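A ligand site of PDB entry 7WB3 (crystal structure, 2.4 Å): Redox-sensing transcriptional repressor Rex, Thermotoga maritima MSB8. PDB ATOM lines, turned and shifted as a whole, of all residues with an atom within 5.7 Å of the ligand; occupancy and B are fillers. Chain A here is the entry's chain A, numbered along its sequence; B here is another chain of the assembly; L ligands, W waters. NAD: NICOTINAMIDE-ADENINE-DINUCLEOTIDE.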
ATOM      1  N   VAL A  88     -26.473  -3.913   8.226  1.00  0.00           N
ATOM      2  CA  VAL A  88     -25.822  -4.000   6.931  1.00  0.00           C
ATOM      3  C   VAL A  88     -24.334  -3.742   7.140  1.00  0.00           C
ATOM      4  O   VAL A  88     -23.939  -2.646   7.549  1.00  0.00           O
ATOM      5  CB  VAL A  88     -26.416  -3.004   5.925  1.00  0.00           C
ATOM      6  CG1 VAL A  88     -25.845  -3.233   4.534  1.00  0.00           C
ATOM      7  CG2 VAL A  88     -27.934  -3.114   5.900  1.00  0.00           C
ATOM      8  N   GLY A  89     -23.520  -4.755   6.868  1.00  0.00           N
ATOM      9  CA  GLY A  89     -22.100  -4.685   7.155  1.00  0.00           C
ATOM     10  C   GLY A  89     -21.743  -5.540   8.352  1.00  0.00           C
ATOM     11  O   GLY A  89     -22.048  -5.180   9.489  1.00  0.00           O
ATOM     12  N   ALA A  90     -21.085  -6.671   8.110  1.00  0.00           N
ATOM     13  CA  ALA A  90     -20.700  -7.608   9.163  1.00  0.00           C
ATOM     14  C   ALA A  90     -19.249  -7.424   9.594  1.00  0.00           C
ATOM     15  O   ALA A  90     -18.581  -8.406   9.941  1.00  0.00           O
ATOM     16  CB  ALA A  90     -20.951  -9.045   8.722  1.00  0.00           C
ATOM     17  N   GLY A  91     -18.740  -6.191   9.580  1.00  0.00           N
ATOM     18  CA  GLY A  91     -17.393  -5.897  10.015  1.00  0.00           C
ATOM     19  C   GLY A  91     -17.295  -5.704  11.510  1.00  0.00           C
ATOM     20  O   GLY A  91     -18.072  -6.263  12.298  1.00  0.00           O
ATOM     21  N   ASN A  92     -16.314  -4.898  11.925  1.00  0.00           N
ATOM     22  CA  ASN A  92     -16.117  -4.626  13.343  1.00  0.00           C
ATOM     23  C   ASN A  92     -17.379  -4.052  13.976  1.00  0.00           C
ATOM     24  O   ASN A  92     -17.917  -4.621  14.930  1.00  0.00           O
ATOM     25  CB  ASN A  92     -14.941  -3.671  13.533  1.00  0.00           C
ATOM     26  CG  ASN A  92     -13.657  -4.187  12.903  1.00  0.00           C
ATOM     27  OD1 ASN A  92     -13.248  -5.332  13.132  1.00  0.00           O
ATOM     28  ND2 ASN A  92     -13.021  -3.353  12.089  1.00  0.00           N
ATOM     29  N   ILE A  93     -17.865  -2.932  13.455  1.00  0.00           N
ATOM     30  CA  ILE A  93     -19.022  -2.270  14.047  1.00  0.00           C
ATOM     31  C   ILE A  93     -20.266  -3.156  13.926  1.00  0.00           C
ATOM     32  O   ILE A  93     -21.012  -3.328  14.890  1.00  0.00           O
ATOM     33  CB  ILE A  93     -19.250  -0.894  13.396  1.00  0.00           C
ATOM     34  CG1 ILE A  93     -18.038   0.013  13.624  1.00  0.00           C
ATOM     35  CG2 ILE A  93     -20.517  -0.257  13.937  1.00  0.00           C
ATOM     36  CD1 ILE A  93     -17.771   0.312  15.077  1.00  0.00           C
ATOM     37  N   GLY A  94     -20.496  -3.714  12.734  1.00  0.00           N
ATOM     38  CA  GLY A  94     -21.692  -4.520  12.531  1.00  0.00           C
ATOM     39  C   GLY A  94     -21.768  -5.700  13.477  1.00  0.00           C
ATOM     40  O   GLY A  94     -22.832  -5.990  14.035  1.00  0.00           O
ATOM     41  N   PHE A 114     -26.316  -8.471   6.991  1.00  0.00           N
ATOM     42  CA  PHE A 114     -26.025  -8.633   5.571  1.00  0.00           C
ATOM     43  C   PHE A 114     -24.617  -8.139   5.266  1.00  0.00           C
ATOM     44  O   PHE A 114     -24.106  -7.206   5.891  1.00  0.00           O
ATOM     45  CB  PHE A 114     -27.043  -7.874   4.721  1.00  0.00           C
ATOM     46  CG  PHE A 114     -28.462  -8.321   4.945  1.00  0.00           C
ATOM     47  CD1 PHE A 114     -29.189  -7.854   6.029  1.00  0.00           C
ATOM     48  CD2 PHE A 114     -29.072  -9.211   4.062  1.00  0.00           C
ATOM     49  CE1 PHE A 114     -30.496  -8.268   6.240  1.00  0.00           C
ATOM     50  CE2 PHE A 114     -30.377  -9.618   4.267  1.00  0.00           C
ATOM     51  CZ  PHE A 114     -31.084  -9.152   5.359  1.00  0.00           C
ATOM     52  N   ASP A 115     -23.993  -8.782   4.281  1.00  0.00           N
ATOM     53  CA  ASP A 115     -22.683  -8.384   3.809  1.00  0.00           C
ATOM     54  C   ASP A 115     -22.574  -8.708   2.325  1.00  0.00           C
ATOM     55  O   ASP A 115     -23.335  -9.527   1.790  1.00  0.00           O
ATOM     56  CB  ASP A 115     -21.563  -9.077   4.600  1.00  0.00           C
ATOM     57  CG  ASP A 115     -20.272  -8.282   4.590  1.00  0.00           C
ATOM     58  OD1 ASP A 115     -19.658  -8.149   3.509  1.00  0.00           O
ATOM     59  OD2 ASP A 115     -19.867  -7.794   5.669  1.00  0.00           O
ATOM     60  N   SER A 116     -21.611  -8.066   1.670  1.00  0.00           N
ATOM     61  CA  SER A 116     -21.358  -8.290   0.252  1.00  0.00           C
ATOM     62  C   SER A 116     -20.108  -9.135   0.002  1.00  0.00           C
ATOM     63  O   SER A 116     -19.833  -9.474  -1.155  1.00  0.00           O
ATOM     64  CB  SER A 116     -21.223  -6.951  -0.472  1.00  0.00           C
ATOM     65  OG  SER A 116     -20.208  -6.155   0.108  1.00  0.00           O
ATOM     66  N   ASP A 117     -19.370  -9.486   1.048  1.00  0.00           N
ATOM     67  CA  ASP A 117     -18.132 -10.230   0.885  1.00  0.00           C
ATOM     68  C   ASP A 117     -18.415 -11.722   0.916  1.00  0.00           C
ATOM     69  O   ASP A 117     -18.876 -12.224   1.947  1.00  0.00           O
ATOM     70  CB  ASP A 117     -17.143  -9.861   1.979  1.00  0.00           C
ATOM     71  CG  ASP A 117     -15.814 -10.587   1.831  1.00  0.00           C
ATOM     72  OD1 ASP A 117     -15.061 -10.265   0.887  1.00  0.00           O
ATOM     73  OD2 ASP A 117     -15.531 -11.482   2.661  1.00  0.00           O
ATOM     74  N   LYS A 120     -17.486 -13.781   4.065  1.00  0.00           N
ATOM     75  CA  LYS A 120     -18.270 -13.696   5.296  1.00  0.00           C
ATOM     76  C   LYS A 120     -19.720 -14.141   5.105  1.00  0.00           C
ATOM     77  O   LYS A 120     -20.378 -14.479   6.086  1.00  0.00           O
ATOM     78  CB  LYS A 120     -18.238 -12.276   5.851  1.00  0.00           C
ATOM     79  CG  LYS A 120     -16.833 -11.768   6.149  1.00  0.00           C
ATOM     80  CD  LYS A 120     -16.860 -10.494   6.975  1.00  0.00           C
ATOM     81  CE  LYS A 120     -17.043  -9.277   6.094  1.00  0.00           C
ATOM     82  NZ  LYS A 120     -15.817  -8.973   5.301  1.00  0.00           N
ATOM     83  N   VAL A 134     -26.000  -9.416   0.839  1.00  0.00           N
ATOM     84  CA  VAL A 134     -26.640  -8.107   0.801  1.00  0.00           C
ATOM     85  C   VAL A 134     -27.608  -7.985  -0.372  1.00  0.00           C
ATOM     86  O   VAL A 134     -28.469  -7.105  -0.372  1.00  0.00           O
ATOM     87  CB  VAL A 134     -25.579  -6.988   0.758  1.00  0.00           C
ATOM     88  CG1 VAL A 134     -24.790  -7.050  -0.548  1.00  0.00           C
ATOM     89  CG2 VAL A 134     -26.237  -5.622   0.921  1.00  0.00           C
ATOM     90  N   ILE A 151     -26.518   0.956   9.417  1.00  0.00           N
ATOM     91  CA  ILE A 151     -25.567   0.994   8.312  1.00  0.00           C
ATOM     92  C   ILE A 151     -24.159   0.940   8.887  1.00  0.00           C
ATOM     93  O   ILE A 151     -23.718   1.875   9.576  1.00  0.00           O
ATOM     94  CB  ILE A 151     -25.767   2.236   7.442  1.00  0.00           C
ATOM     95  CG1 ILE A 151     -27.177   2.238   6.826  1.00  0.00           C
ATOM     96  CG2 ILE A 151     -24.708   2.297   6.347  1.00  0.00           C
ATOM     97  CD1 ILE A 151     -27.474   3.453   5.981  1.00  0.00           C
ATOM     98  N   ALA A 152     -23.450  -0.149   8.604  1.00  0.00           N
ATOM     99  CA  ALA A 152     -22.066  -0.344   9.036  1.00  0.00           C
ATOM    100  C   ALA A 152     -21.195  -0.742   7.843  1.00  0.00           C
ATOM    101  O   ALA A 152     -20.381  -1.671   7.914  1.00  0.00           O
ATOM    102  CB  ALA A 152     -21.983  -1.388  10.142  1.00  0.00           C
ATOM    103  N   VAL A 153     -21.369  -0.032   6.736  1.00  0.00           N
ATOM    104  CA  VAL A 153     -20.566  -0.266   5.534  1.00  0.00           C
ATOM    105  C   VAL A 153     -19.645   0.943   5.341  1.00  0.00           C
ATOM    106  O   VAL A 153     -19.914   2.013   5.905  1.00  0.00           O
ATOM    107  CB  VAL A 153     -21.441  -0.493   4.295  1.00  0.00           C
ATOM    108  CG1 VAL A 153     -22.402  -1.647   4.532  1.00  0.00           C
ATOM    109  CG2 VAL A 153     -22.192   0.788   3.928  1.00  0.00           C
ATOM    110  N   PRO A 154     -18.572   0.821   4.570  1.00  0.00           N
ATOM    111  CA  PRO A 154     -17.704   1.978   4.313  1.00  0.00           C
ATOM    112  C   PRO A 154     -18.487   3.160   3.768  1.00  0.00           C
ATOM    113  O   PRO A 154     -19.567   2.977   3.195  1.00  0.00           O
ATOM    114  CB  PRO A 154     -16.691   1.446   3.299  1.00  0.00           C
ATOM    115  CG  PRO A 154     -16.646  -0.031   3.556  1.00  0.00           C
ATOM    116  CD  PRO A 154     -18.051  -0.406   3.927  1.00  0.00           C
ATOM    117  N   ALA A 155     -17.957   4.365   3.940  1.00  0.00           N
ATOM    118  CA  ALA A 155     -18.690   5.571   3.562  1.00  0.00           C
ATOM    119  C   ALA A 155     -19.103   5.531   2.093  1.00  0.00           C
ATOM    120  O   ALA A 155     -20.191   6.003   1.744  1.00  0.00           O
ATOM    121  CB  ALA A 155     -17.847   6.807   3.849  1.00  0.00           C
ATOM    122  N   HIS A 157     -20.335   3.408   0.300  1.00  0.00           N
ATOM    123  CA  HIS A 157     -21.530   2.630   0.011  1.00  0.00           C
ATOM    124  C   HIS A 157     -22.669   2.905   0.975  1.00  0.00           C
ATOM    125  O   HIS A 157     -23.688   2.209   0.923  1.00  0.00           O
ATOM    126  CB  HIS A 157     -21.196   1.137   0.009  1.00  0.00           C
ATOM    127  CG  HIS A 157     -20.213   0.736  -1.047  1.00  0.00           C
ATOM    128  ND1 HIS A 157     -19.281  -0.268  -0.868  1.00  0.00           N
ATOM    129  CD2 HIS A 157     -20.009   1.213  -2.303  1.00  0.00           C
ATOM    130  CE1 HIS A 157     -18.557  -0.398  -1.954  1.00  0.00           C
ATOM    131  NE2 HIS A 157     -18.976   0.487  -2.843  1.00  0.00           N
ATOM    132  N   ILE A 161     -26.812   2.060   0.300  1.00  0.00           N
ATOM    133  CA  ILE A 161     -27.510   1.158   1.207  1.00  0.00           C
ATOM    134  C   ILE A 161     -28.696   1.864   1.848  1.00  0.00           C
ATOM    135  O   ILE A 161     -29.759   1.262   2.078  1.00  0.00           O
ATOM    136  CB  ILE A 161     -26.538   0.610   2.270  1.00  0.00           C
ATOM    137  CG1 ILE A 161     -25.565  -0.385   1.640  1.00  0.00           C
ATOM    138  CG2 ILE A 161     -27.315  -0.033   3.410  1.00  0.00           C
ATOM    139  CD1 ILE A 161     -26.233  -1.590   1.021  1.00  0.00           C
ATOM    140  N   ARG A 164     -31.680   1.808  -0.587  1.00  0.00           N
ATOM    141  CA  ARG A 164     -32.337   0.501  -0.691  1.00  0.00           C
ATOM    142  C   ARG A 164     -33.222   0.233   0.509  1.00  0.00           C
ATOM    143  O   ARG A 164     -34.353  -0.267   0.363  1.00  0.00           O
ATOM    144  CB  ARG A 164     -31.283  -0.597  -0.851  1.00  0.00           C
ATOM    145  CG  ARG A 164     -30.533  -0.531  -2.170  1.00  0.00           C
ATOM    146  CD  ARG A 164     -29.473  -1.612  -2.265  1.00  0.00           C
ATOM    147  NE  ARG A 164     -28.654  -1.458  -3.461  1.00  0.00           N
ATOM    148  CZ  ARG A 164     -27.669  -2.285  -3.803  1.00  0.00           C
ATOM    149  NH1 ARG A 164     -27.381  -3.326  -3.038  1.00  0.00           N
ATOM    150  NH2 ARG A 164     -26.964  -2.059  -4.909  1.00  0.00           N
ATOM    151  N   PHE A 176     -23.506   4.599  10.946  1.00  0.00           N
ATOM    152  CA  PHE A 176     -22.165   4.650  11.499  1.00  0.00           C
ATOM    153  C   PHE A 176     -21.125   5.200  10.525  1.00  0.00           C
ATOM    154  O   PHE A 176     -20.030   5.569  10.956  1.00  0.00           O
ATOM    155  CB  PHE A 176     -21.711   3.262  11.961  1.00  0.00           C
ATOM    156  CG  PHE A 176     -22.265   2.848  13.298  1.00  0.00           C
ATOM    157  CD1 PHE A 176     -23.465   2.175  13.381  1.00  0.00           C
ATOM    158  CD2 PHE A 176     -21.564   3.113  14.458  1.00  0.00           C
ATOM    159  CE1 PHE A 176     -23.974   1.787  14.612  1.00  0.00           C
ATOM    160  CE2 PHE A 176     -22.063   2.735  15.690  1.00  0.00           C
ATOM    161  CZ  PHE A 176     -23.261   2.070  15.768  1.00  0.00           C
ATOM    162  N   ALA A 177     -21.446   5.262   9.228  1.00  0.00           N
ATOM    163  CA  ALA A 177     -20.465   5.655   8.218  1.00  0.00           C
ATOM    164  C   ALA A 177     -20.240   7.168   8.246  1.00  0.00           C
ATOM    165  O   ALA A 177     -21.204   7.939   8.352  1.00  0.00           O
ATOM    166  CB  ALA A 177     -20.916   5.231   6.828  1.00  0.00           C
ATOM    167  N   PRO A 178     -18.997   7.617   8.112  1.00  0.00           N
ATOM    168  CA  PRO A 178     -18.722   9.057   8.201  1.00  0.00           C
ATOM    169  C   PRO A 178     -19.166   9.813   6.950  1.00  0.00           C
ATOM    170  O   PRO A 178     -18.328  10.338   6.213  1.00  0.00           O
ATOM    171  CB  PRO A 178     -17.196   9.105   8.376  1.00  0.00           C
ATOM    172  CG  PRO A 178     -16.711   7.882   7.649  1.00  0.00           C
ATOM    173  CD  PRO A 178     -17.776   6.830   7.860  1.00  0.00           C
ATOM    174  N   ASP A 191     -20.753   9.089  14.603  1.00  0.00           N
ATOM    175  CA  ASP A 191     -19.502   9.284  13.880  1.00  0.00           C
ATOM    176  C   ASP A 191     -18.350   9.227  14.884  1.00  0.00           C
ATOM    177  O   ASP A 191     -18.038  10.221  15.545  1.00  0.00           O
ATOM    178  CB  ASP A 191     -19.515  10.602  13.114  1.00  0.00           C
ATOM    179  CG  ASP A 191     -18.401  10.702  12.082  1.00  0.00           C
ATOM    180  OD1 ASP A 191     -17.341  10.073  12.300  1.00  0.00           O
ATOM    181  OD2 ASP A 191     -18.589  11.386  11.061  1.00  0.00           O
ATOM    182  N   ILE A 192     -17.733   8.051  14.998  1.00  0.00           N
ATOM    183  CA  ILE A 192     -16.708   7.841  16.012  1.00  0.00           C
ATOM    184  C   ILE A 192     -15.519   8.773  15.793  1.00  0.00           C
ATOM    185  O   ILE A 192     -15.028   9.410  16.725  1.00  0.00           O
ATOM    186  CB  ILE A 192     -16.271   6.363  16.043  1.00  0.00           C
ATOM    187  CG1 ILE A 192     -17.414   5.484  16.563  1.00  0.00           C
ATOM    188  CG2 ILE A 192     -15.011   6.188  16.887  1.00  0.00           C
ATOM    189  CD1 ILE A 192     -17.129   3.998  16.475  1.00  0.00           C
ATOM    190  N   THR A 193     -15.044   8.850  14.548  1.00  0.00           N
ATOM    191  CA  THR A 193     -13.891   9.705  14.272  1.00  0.00           C
ATOM    192  C   THR A 193     -14.211  11.169  14.548  1.00  0.00           C
ATOM    193  O   THR A 193     -13.370  11.900  15.083  1.00  0.00           O
ATOM    194  CB  THR A 193     -13.428   9.519  12.821  1.00  0.00           C
ATOM    195  OG1 THR A 193     -12.934   8.194  12.644  1.00  0.00           O
ATOM    196  CG2 THR A 193     -12.323  10.514  12.490  1.00  0.00           C
ATOM    197  N   ALA B  96     -13.571  -3.557  18.101  1.00  0.00           N
ATOM    198  CA  ALA B  96     -13.965  -2.860  16.875  1.00  0.00           C
ATOM    199  C   ALA B  96     -13.186  -1.567  16.706  1.00  0.00           C
ATOM    200  O   ALA B  96     -12.742  -1.247  15.601  1.00  0.00           O
ATOM    201  CB  ALA B  96     -15.464  -2.589  16.887  1.00  0.00           C
ATOM    202  N   VAL B  97     -12.999  -0.809  17.787  1.00  0.00           N
ATOM    203  CA  VAL B  97     -12.267   0.443  17.700  1.00  0.00           C
ATOM    204  C   VAL B  97     -10.773   0.191  17.532  1.00  0.00           C
ATOM    205  O   VAL B  97     -10.085   0.908  16.807  1.00  0.00           O
ATOM    206  CB  VAL B  97     -12.551   1.325  18.933  1.00  0.00           C
ATOM    207  CG1 VAL B  97     -11.644   2.547  18.936  1.00  0.00           C
ATOM    208  CG2 VAL B  97     -14.017   1.731  18.955  1.00  0.00           C
ATOM    209  N   TYR B 100      -9.945  -0.828  13.951  1.00  0.00           N
ATOM    210  CA  TYR B 100     -10.130   0.270  13.004  1.00  0.00           C
ATOM    211  C   TYR B 100      -9.004   1.291  13.105  1.00  0.00           C
ATOM    212  O   TYR B 100      -8.402   1.657  12.084  1.00  0.00           O
ATOM    213  CB  TYR B 100     -11.486   0.952  13.242  1.00  0.00           C
ATOM    214  CG  TYR B 100     -11.777   2.049  12.246  1.00  0.00           C
ATOM    215  CD1 TYR B 100     -12.433   1.774  11.055  1.00  0.00           C
ATOM    216  CD2 TYR B 100     -11.378   3.364  12.484  1.00  0.00           C
ATOM    217  CE1 TYR B 100     -12.696   2.776  10.135  1.00  0.00           C
ATOM    218  CE2 TYR B 100     -11.643   4.366  11.581  1.00  0.00           C
ATOM    219  CZ  TYR B 100     -12.306   4.067  10.407  1.00  0.00           C
ATOM    220  OH  TYR B 100     -12.569   5.070   9.487  1.00  0.00           O
ATOM    221  N   LYS B 104      -7.284   2.176   9.749  1.00  0.00           N
ATOM    222  CA  LYS B 104      -7.803   3.276   8.947  1.00  0.00           C
ATOM    223  C   LYS B 104      -7.305   4.644   9.380  1.00  0.00           C
ATOM    224  O   LYS B 104      -7.163   5.535   8.535  1.00  0.00           O
ATOM    225  CB  LYS B 104      -9.334   3.273   8.964  1.00  0.00           C
ATOM    226  CG  LYS B 104      -9.963   2.064   8.301  1.00  0.00           C
ATOM    227  CD  LYS B 104      -9.664   2.029   6.814  1.00  0.00           C
ATOM    228  CE  LYS B 104     -10.381   0.868   6.128  1.00  0.00           C
ATOM    229  NZ  LYS B 104     -10.137   0.854   4.665  1.00  0.00           N
HETATM  230  PA  NAD L   1     -15.224  -3.113   8.392  1.00  0.00           P
HETATM  231  O1A NAD L   1     -14.211  -3.169   7.234  1.00  0.00           O
HETATM  232  O2A NAD L   1     -14.679  -3.848   9.630  1.00  0.00           O
HETATM  233  O5B NAD L   1     -16.656  -3.814   7.927  1.00  0.00           O
HETATM  234  C5B NAD L   1     -17.377  -3.186   6.893  1.00  0.00           C
HETATM  235  C4B NAD L   1     -18.232  -4.270   6.166  1.00  0.00           C
HETATM  236  O4B NAD L   1     -19.000  -3.698   5.266  1.00  0.00           O
HETATM  237  C3B NAD L   1     -17.312  -5.229   5.399  1.00  0.00           C
HETATM  238  O3B NAD L   1     -17.418  -6.496   5.912  1.00  0.00           O
HETATM  239  C2B NAD L   1     -17.798  -5.179   3.938  1.00  0.00           C
HETATM  240  O2B NAD L   1     -17.796  -6.561   3.346  1.00  0.00           O
HETATM  241  C1B NAD L   1     -19.023  -4.726   4.028  1.00  0.00           C
HETATM  242  N9A NAD L   1     -19.489  -4.013   2.831  1.00  0.00           N
HETATM  243  C8A NAD L   1     -18.841  -3.161   2.030  1.00  0.00           C
HETATM  244  N7A NAD L   1     -19.692  -2.760   1.080  1.00  0.00           N
HETATM  245  C5A NAD L   1     -20.871  -3.359   1.299  1.00  0.00           C
HETATM  246  C6A NAD L   1     -22.088  -3.302   0.631  1.00  0.00           C
HETATM  247  N6A NAD L   1     -22.571  -2.593  -0.544  1.00  0.00           N
HETATM  248  N1A NAD L   1     -23.112  -4.001   1.065  1.00  0.00           N
HETATM  249  C2A NAD L   1     -22.990  -4.777   2.161  1.00  0.00           C
HETATM  250  N3A NAD L   1     -21.804  -4.843   2.820  1.00  0.00           N
HETATM  251  C4A NAD L   1     -20.751  -4.121   2.377  1.00  0.00           C
HETATM  252  O3  NAD L   1     -15.528  -1.541   8.798  1.00  0.00           O
HETATM  253  PN  NAD L   1     -16.020  -1.126  10.314  1.00  0.00           P
HETATM  254  O1N NAD L   1     -14.820  -1.001  11.203  1.00  0.00           O
HETATM  255  O2N NAD L   1     -16.905  -2.174  10.831  1.00  0.00           O
HETATM  256  O5D NAD L   1     -16.837   0.324  10.273  1.00  0.00           O
HETATM  257  C5D NAD L   1     -18.011   0.436   9.523  1.00  0.00           C
HETATM  258  C4D NAD L   1     -18.328   1.954   9.312  1.00  0.00           C
HETATM  259  O4D NAD L   1     -18.120   2.600  10.423  1.00  0.00           O
HETATM  260  C3D NAD L   1     -17.356   2.557   8.258  1.00  0.00           C
HETATM  261  O3D NAD L   1     -17.999   3.453   7.448  1.00  0.00           O
HETATM  262  C2D NAD L   1     -16.303   3.272   9.101  1.00  0.00           C
HETATM  263  O2D NAD L   1     -15.707   4.426   8.334  1.00  0.00           O
HETATM  264  C1D NAD L   1     -16.970   3.704  10.144  1.00  0.00           C
HETATM  265  N1N NAD L   1     -16.088   3.844  11.296  1.00  0.00           N
HETATM  266  C2N NAD L   1     -15.803   2.773  12.089  1.00  0.00           C
HETATM  267  C3N NAD L   1     -14.954   2.932  13.179  1.00  0.00           C
HETATM  268  C7N NAD L   1     -14.605   1.719  14.087  1.00  0.00           C
HETATM  269  O7N NAD L   1     -14.371   1.887  15.205  1.00  0.00           O
HETATM  270  N7N NAD L   1     -14.570   0.362  13.527  1.00  0.00           N
HETATM  271  C4N NAD L   1     -14.421   4.125  13.445  1.00  0.00           C
HETATM  272  C5N NAD L   1     -14.715   5.193  12.662  1.00  0.00           C
HETATM  273  C6N NAD L   1     -15.553   5.044  11.573  1.00  0.00           C
HETATM  274  O   HOH W   1     -14.708  -3.448   4.301  1.00  0.00           O
HETATM  275  O   HOH W   2     -16.296   7.919  12.039  1.00  0.00           O
HETATM  276  O   HOH W   3     -19.483  -3.336  10.254  1.00  0.00           O
HETATM  277  O   HOH W   4     -13.698  -6.220   8.618  1.00  0.00           O
HETATM  278  O   HOH W   5     -18.330   5.879  12.981  1.00  0.00           O
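The backbone NH of Thr 193 sits close to the side-chain carboxylate of Asp 191, at 3.4 Å. The backbone carbonyl oxygen (O) of Asp 115 lies within hydrogen-bond range of the backbone NH (N) of Val 134 (2.8 Å). OD2 of Asp 117 lies within salt-bridge range of NZ of Lys 120, at 3.7 Å. N of Phe 176 sits at hydrogen-bond distance from O of Ile 151 (3.1 Å). The backbone NH (N) of Ala 90 lies within hydrogen-bond range of the side-chain carboxylate (OD2) of Asp 115, at 3.0 Å. N of Gly 89 sits at hydrogen-bond distance from O of Phe 114, 2.7 Å away. OD1 of Asp 115 sits at hydrogen-bond distance from N of Asp 117 (2.8 Å). O of Val 88 is in hydrogen-bond range of N of Ala 152 (2.8 Å).
Water W3 lies within hydrogen-bond range of the backbone NH of Gly 94 (2.7 Å), an oxygen (O2N) of the ligand (2.9 Å), the backbone carbonyl oxygen of Ala 152 (3.0 Å), the backbone NH of Gly 91 (3.0 Å) and the backbone carbonyl oxygen of Gly 89 (3.3 Å). Water W2 lies within hydrogen-bond range of the side-chain carboxylate of Asp 191 (2.4 Å), the backbone NH of Thr 193 (3.0 Å) and the backbone NH of Ile 192 (3.3 Å). Water W5 bridges O of Phe 176 (2.7 Å) and N of Ile 192 (3.0 Å).
O3B of the ligand lies close to NZ of Lys 120 (3.0 Å). An oxygen (O2D) of the ligand lies within hydrogen-bond range of the side-chain hydroxyl of Tyr 100 of chain B (3.4 Å). The backbone NH (N) of Ile 93 lies within hydrogen-bond range of an oxygen (O2N) of the ligand (2.9 Å). A nitrogen (N3A) of the ligand sits at hydrogen-bond distance from the backbone NH (N) of Ser 116 (3.4 Å). ND2 of Asn 92 is in hydrogen-bond range of O2A of the ligand, 3.0 Å away. O of Val 153 is in hydrogen-bond range of O3D of the ligand, at 2.8 Å. O of Ala 96 of chain B lies within hydrogen-bond range of N7N of the ligand (3.2 Å). The side-chain hydroxyl (OG) of Ser 116 lies close to a nitrogen (N3A) of the ligand, 3.4 Å away. A nitrogen (N7A) of the ligand is in hydrogen-bond range of a ring nitrogen (ND1) of His 157 (3.2 Å). The backbone NH (N) of Asn 92 lies within hydrogen-bond range of an oxygen (O2N) of the ligand. An oxygen (O2B) of the ligand sits at hydrogen-bond distance from the side-chain carboxylate (OD1) of Asp 115, at 2.5 Å.
Merely in contact with the ligand: Gly 91 (3.0 Å), Pro 178 (3.2 Å), Ala 177 (3.4 Å), Pro 154 (3.4 Å), Thr 193 (3.5 Å), Ala 152 (3.5 Å), Val 134 (3.5 Å), Val 97 of chain B (3.6 Å), Phe 176 (3.6 Å), Ala 155 (3.6 Å), Asp 117 (3.6 Å), Ile 192 (3.7 Å), Gly 89 (3.8 Å) and Ile 161 (3.9 Å). Hydrophobic or aromatic side chains that line the ligand: Ile 93, Val 134, Val 153, Pro 154, Ile 161, Phe 176, Ala 177, Pro 178, Ile 192, Val 97 of chain B and Tyr 100 of chain B. Within 4 Å of the ligand: Gly 89, Gly 91, Asn 92, Ile 93, Asp 115, Ser 116, Asp 117, Lys 120, Val 134, Ala 152, Val 153, Pro 154, Ala 155, His 157, Ile 161, Phe 176, Ala 177, Pro 178, Ile 192, Thr 193, Ala 96 of chain B, Val 97 of chain B and Tyr 100 of chain B.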
